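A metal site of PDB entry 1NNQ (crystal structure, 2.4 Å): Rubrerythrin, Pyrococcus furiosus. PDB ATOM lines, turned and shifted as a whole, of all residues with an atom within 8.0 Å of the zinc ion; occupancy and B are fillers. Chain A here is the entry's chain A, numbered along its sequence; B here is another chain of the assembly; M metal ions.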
ATOM      1  N   TYR A 109      -0.768 -15.783  25.392  1.00  0.00           N
ATOM      2  CA  TYR A 109      -0.455 -14.424  25.849  1.00  0.00           C
ATOM      3  C   TYR A 109      -0.027 -14.457  27.325  1.00  0.00           C
ATOM      4  O   TYR A 109       0.990 -13.936  27.692  1.00  0.00           O
ATOM      5  CB  TYR A 109      -1.649 -13.483  25.607  1.00  0.00           C
ATOM      6  CG  TYR A 109      -1.803 -12.947  24.191  1.00  0.00           C
ATOM      7  CD1 TYR A 109      -0.919 -13.325  23.164  1.00  0.00           C
ATOM      8  CD2 TYR A 109      -2.829 -12.048  23.871  1.00  0.00           C
ATOM      9  CE1 TYR A 109      -1.062 -12.817  21.867  1.00  0.00           C
ATOM     10  CE2 TYR A 109      -2.980 -11.537  22.568  1.00  0.00           C
ATOM     11  CZ  TYR A 109      -2.101 -11.937  21.576  1.00  0.00           C
ATOM     12  OH  TYR A 109      -2.233 -11.431  20.298  1.00  0.00           O
ATOM     13  N   ILE A 141       3.918  -2.324  30.458  1.00  0.00           N
ATOM     14  CA  ILE A 141       3.012  -3.447  30.247  1.00  0.00           C
ATOM     15  C   ILE A 141       2.261  -3.332  28.911  1.00  0.00           C
ATOM     16  O   ILE A 141       1.573  -2.343  28.685  1.00  0.00           O
ATOM     17  CB  ILE A 141       1.964  -3.550  31.404  1.00  0.00           C
ATOM     18  CG1 ILE A 141       2.577  -3.333  32.821  1.00  0.00           C
ATOM     19  CG2 ILE A 141       1.154  -4.849  31.262  1.00  0.00           C
ATOM     20  CD1 ILE A 141       3.557  -4.403  33.296  1.00  0.00           C
ATOM     21  N   CYS A 142       2.355  -4.340  28.050  1.00  0.00           N
ATOM     22  CA  CYS A 142       1.531  -4.358  26.847  1.00  0.00           C
ATOM     23  C   CYS A 142       0.063  -4.601  27.237  1.00  0.00           C
ATOM     24  O   CYS A 142      -0.223  -5.599  27.892  1.00  0.00           O
ATOM     25  CB  CYS A 142       2.020  -5.412  25.843  1.00  0.00           C
ATOM     26  SG  CYS A 142       1.008  -5.573  24.326  1.00  0.00           S
ATOM     27  N   PRO A 143      -0.828  -3.686  26.848  1.00  0.00           N
ATOM     28  CA  PRO A 143      -2.254  -3.793  27.204  1.00  0.00           C
ATOM     29  C   PRO A 143      -3.007  -4.800  26.337  1.00  0.00           C
ATOM     30  O   PRO A 143      -4.198  -5.013  26.583  1.00  0.00           O
ATOM     31  CB  PRO A 143      -2.770  -2.369  26.965  1.00  0.00           C
ATOM     32  CG  PRO A 143      -1.943  -1.910  25.711  1.00  0.00           C
ATOM     33  CD  PRO A 143      -0.552  -2.485  26.023  1.00  0.00           C
ATOM     34  N   ILE A 144      -2.345  -5.442  25.383  1.00  0.00           N
ATOM     35  CA  ILE A 144      -2.961  -6.498  24.551  1.00  0.00           C
ATOM     36  C   ILE A 144      -2.636  -7.874  25.104  1.00  0.00           C
ATOM     37  O   ILE A 144      -3.509  -8.742  25.274  1.00  0.00           O
ATOM     38  CB  ILE A 144      -2.431  -6.409  23.101  1.00  0.00           C
ATOM     39  CG1 ILE A 144      -2.626  -5.007  22.510  1.00  0.00           C
ATOM     40  CG2 ILE A 144      -3.041  -7.504  22.193  1.00  0.00           C
ATOM     41  CD1 ILE A 144      -4.116  -4.581  22.364  1.00  0.00           C
ATOM     42  N   CYS A 145      -1.359  -8.109  25.393  1.00  0.00           N
ATOM     43  CA  CYS A 145      -0.958  -9.433  25.798  1.00  0.00           C
ATOM     44  C   CYS A 145      -0.340  -9.492  27.185  1.00  0.00           C
ATOM     45  O   CYS A 145      -0.050 -10.572  27.674  1.00  0.00           O
ATOM     46  CB  CYS A 145      -0.006  -9.999  24.751  1.00  0.00           C
ATOM     47  SG  CYS A 145       1.635  -9.281  24.886  1.00  0.00           S
ATOM     48  N   GLY A 146      -0.100  -8.350  27.821  1.00  0.00           N
ATOM     49  CA  GLY A 146       0.470  -8.336  29.157  1.00  0.00           C
ATOM     50  C   GLY A 146       1.970  -8.549  29.290  1.00  0.00           C
ATOM     51  O   GLY A 146       2.483  -8.648  30.419  1.00  0.00           O
ATOM     52  N   TYR A 147       2.663  -8.628  28.156  1.00  0.00           N
ATOM     53  CA  TYR A 147       4.126  -8.581  28.106  1.00  0.00           C
ATOM     54  C   TYR A 147       4.651  -7.468  29.017  1.00  0.00           C
ATOM     55  O   TYR A 147       4.106  -6.366  29.055  1.00  0.00           O
ATOM     56  CB  TYR A 147       4.615  -8.372  26.666  1.00  0.00           C
ATOM     57  CG  TYR A 147       6.092  -7.968  26.555  1.00  0.00           C
ATOM     58  CD1 TYR A 147       6.464  -6.620  26.452  1.00  0.00           C
ATOM     59  CD2 TYR A 147       7.100  -8.953  26.547  1.00  0.00           C
ATOM     60  CE1 TYR A 147       7.831  -6.255  26.344  1.00  0.00           C
ATOM     61  CE2 TYR A 147       8.462  -8.598  26.461  1.00  0.00           C
ATOM     62  CZ  TYR A 147       8.813  -7.245  26.355  1.00  0.00           C
ATOM     63  OH  TYR A 147      10.148  -6.894  26.252  1.00  0.00           O
ATOM     64  N   THR A 148       5.737  -7.771  29.726  1.00  0.00           N
ATOM     65  CA  THR A 148       6.219  -6.952  30.818  1.00  0.00           C
ATOM     66  C   THR A 148       7.727  -6.655  30.642  1.00  0.00           C
ATOM     67  O   THR A 148       8.518  -7.568  30.471  1.00  0.00           O
ATOM     68  CB  THR A 148       5.985  -7.720  32.109  1.00  0.00           C
ATOM     69  OG1 THR A 148       4.575  -7.976  32.262  1.00  0.00           O
ATOM     70  CG2 THR A 148       6.362  -6.874  33.308  1.00  0.00           C
ATOM     71  N   TYR A 156       8.442  -2.828  19.537  1.00  0.00           N
ATOM     72  CA  TYR A 156       7.222  -3.589  19.312  1.00  0.00           C
ATOM     73  C   TYR A 156       7.210  -4.708  20.303  1.00  0.00           C
ATOM     74  O   TYR A 156       8.253  -5.294  20.615  1.00  0.00           O
ATOM     75  CB  TYR A 156       7.164  -4.135  17.873  1.00  0.00           C
ATOM     76  CG  TYR A 156       7.042  -3.008  16.865  1.00  0.00           C
ATOM     77  CD1 TYR A 156       5.796  -2.501  16.498  1.00  0.00           C
ATOM     78  CD2 TYR A 156       8.197  -2.408  16.317  1.00  0.00           C
ATOM     79  CE1 TYR A 156       5.667  -1.449  15.601  1.00  0.00           C
ATOM     80  CE2 TYR A 156       8.091  -1.340  15.410  1.00  0.00           C
ATOM     81  CZ  TYR A 156       6.820  -0.870  15.067  1.00  0.00           C
ATOM     82  OH  TYR A 156       6.675   0.176  14.172  1.00  0.00           O
ATOM     83  N   CYS A 157       6.022  -5.004  20.822  1.00  0.00           N
ATOM     84  CA  CYS A 157       5.827  -6.142  21.694  1.00  0.00           C
ATOM     85  C   CYS A 157       6.260  -7.399  20.973  1.00  0.00           C
ATOM     86  O   CYS A 157       5.796  -7.680  19.877  1.00  0.00           O
ATOM     87  CB  CYS A 157       4.352  -6.251  22.102  1.00  0.00           C
ATOM     88  SG  CYS A 157       4.011  -7.673  23.182  1.00  0.00           S
ATOM     89  N   PRO A 158       7.171  -8.162  21.564  1.00  0.00           N
ATOM     90  CA  PRO A 158       7.634  -9.398  20.933  1.00  0.00           C
ATOM     91  C   PRO A 158       6.561 -10.504  20.899  1.00  0.00           C
ATOM     92  O   PRO A 158       6.777 -11.513  20.202  1.00  0.00           O
ATOM     93  CB  PRO A 158       8.777  -9.844  21.851  1.00  0.00           C
ATOM     94  CG  PRO A 158       8.463  -9.248  23.184  1.00  0.00           C
ATOM     95  CD  PRO A 158       7.804  -7.914  22.871  1.00  0.00           C
ATOM     96  N   VAL A 159       5.458 -10.335  21.633  1.00  0.00           N
ATOM     97  CA  VAL A 159       4.438 -11.392  21.665  1.00  0.00           C
ATOM     98  C   VAL A 159       3.312 -11.110  20.666  1.00  0.00           C
ATOM     99  O   VAL A 159       2.983 -11.972  19.860  1.00  0.00           O
ATOM    100  CB  VAL A 159       3.887 -11.681  23.096  1.00  0.00           C
ATOM    101  CG1 VAL A 159       2.813 -12.755  23.058  1.00  0.00           C
ATOM    102  CG2 VAL A 159       5.021 -12.094  24.041  1.00  0.00           C
ATOM    103  N   CYS A 160       2.770  -9.896  20.719  1.00  0.00           N
ATOM    104  CA  CYS A 160       1.608  -9.552  19.883  1.00  0.00           C
ATOM    105  C   CYS A 160       1.903  -8.529  18.787  1.00  0.00           C
ATOM    106  O   CYS A 160       1.042  -8.307  17.921  1.00  0.00           O
ATOM    107  CB  CYS A 160       0.454  -9.041  20.754  1.00  0.00           C
ATOM    108  SG  CYS A 160       0.675  -7.375  21.434  1.00  0.00           S
ATOM    109  N   GLY A 161       3.074  -7.883  18.811  1.00  0.00           N
ATOM    110  CA  GLY A 161       3.422  -6.904  17.803  1.00  0.00           C
ATOM    111  C   GLY A 161       2.968  -5.461  18.059  1.00  0.00           C
ATOM    112  O   GLY A 161       3.345  -4.590  17.298  1.00  0.00           O
ATOM    113  N   ALA A 162       2.213  -5.213  19.124  1.00  0.00           N
ATOM    114  CA  ALA A 162       1.813  -3.847  19.508  1.00  0.00           C
ATOM    115  C   ALA A 162       2.999  -2.882  19.654  1.00  0.00           C
ATOM    116  O   ALA A 162       4.066  -3.284  20.121  1.00  0.00           O
ATOM    117  CB  ALA A 162       0.993  -3.849  20.782  1.00  0.00           C
ATOM    118  N   PRO A 163       2.808  -1.622  19.261  1.00  0.00           N
ATOM    119  CA  PRO A 163       3.891  -0.632  19.314  1.00  0.00           C
ATOM    120  C   PRO A 163       4.124  -0.142  20.729  1.00  0.00           C
ATOM    121  O   PRO A 163       3.165  -0.035  21.504  1.00  0.00           O
ATOM    122  CB  PRO A 163       3.377   0.541  18.427  1.00  0.00           C
ATOM    123  CG  PRO A 163       1.990   0.152  17.923  1.00  0.00           C
ATOM    124  CD  PRO A 163       1.555  -1.065  18.705  1.00  0.00           C
ATOM    125  N   PHE A 167       2.206   0.899  25.216  1.00  0.00           N
ATOM    126  CA  PHE A 167       2.509   0.287  26.497  1.00  0.00           C
ATOM    127  C   PHE A 167       2.015   1.140  27.674  1.00  0.00           C
ATOM    128  O   PHE A 167       2.062   2.379  27.632  1.00  0.00           O
ATOM    129  CB  PHE A 167       3.999  -0.038  26.658  1.00  0.00           C
ATOM    130  CG  PHE A 167       4.536  -1.040  25.656  1.00  0.00           C
ATOM    131  CD1 PHE A 167       3.686  -1.750  24.780  1.00  0.00           C
ATOM    132  CD2 PHE A 167       5.915  -1.261  25.565  1.00  0.00           C
ATOM    133  CE1 PHE A 167       4.185  -2.656  23.864  1.00  0.00           C
ATOM    134  CE2 PHE A 167       6.434  -2.181  24.652  1.00  0.00           C
ATOM    135  CZ  PHE A 167       5.567  -2.878  23.787  1.00  0.00           C
ATOM    136  N   VAL B  54      -4.850  -7.605  32.380  1.00  0.00           N
ATOM    137  CA  VAL B  54      -4.875  -7.830  30.931  1.00  0.00           C
ATOM    138  C   VAL B  54      -5.233  -9.297  30.610  1.00  0.00           C
ATOM    139  O   VAL B  54      -6.095  -9.546  29.765  1.00  0.00           O
ATOM    140  CB  VAL B  54      -3.570  -7.378  30.221  1.00  0.00           C
ATOM    141  CG1 VAL B  54      -3.590  -7.714  28.726  1.00  0.00           C
ATOM    142  CG2 VAL B  54      -3.378  -5.860  30.367  1.00  0.00           C
HETATM  143 ZN    ZN M   1       1.757  -7.493  23.457  1.00  0.00          ZN
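Four residues have an atom within 4 Å of the zinc ion: Cys 142, Cys 145, Cys 157 and Cys 160. Along chain A the residues within 4 Å of the zinc ion span positions 142 to 160.
The zinc ion is bound by the side-chain sulfur of Cys 142, the side-chain sulfur of Cys 157, the side-chain sulfur of Cys 145 and the side-chain sulfur of Cys 160. The zinc ion has four donor atoms within binding distance.
N of Cys 157 sits at hydrogen-bond distance from O of Ala 162 (2.7 Å). The side-chain sulfur (SG) of Cys 145 sits close to the backbone NH (N) of Tyr 147 (3.5 Å). The side-chain sulfur of Cys 160 sits close to the backbone NH of Ala 162 (3.5 Å). The backbone NH of Val 159 lies close to the side-chain sulfur of Cys 157 (3.4 Å). The backbone NH (N) of Cys 142 sits at hydrogen-bond distance from the backbone carbonyl oxygen (O) of Tyr 147. SG of Cys 142 sits close to N of Ile 144 (3.5 Å).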
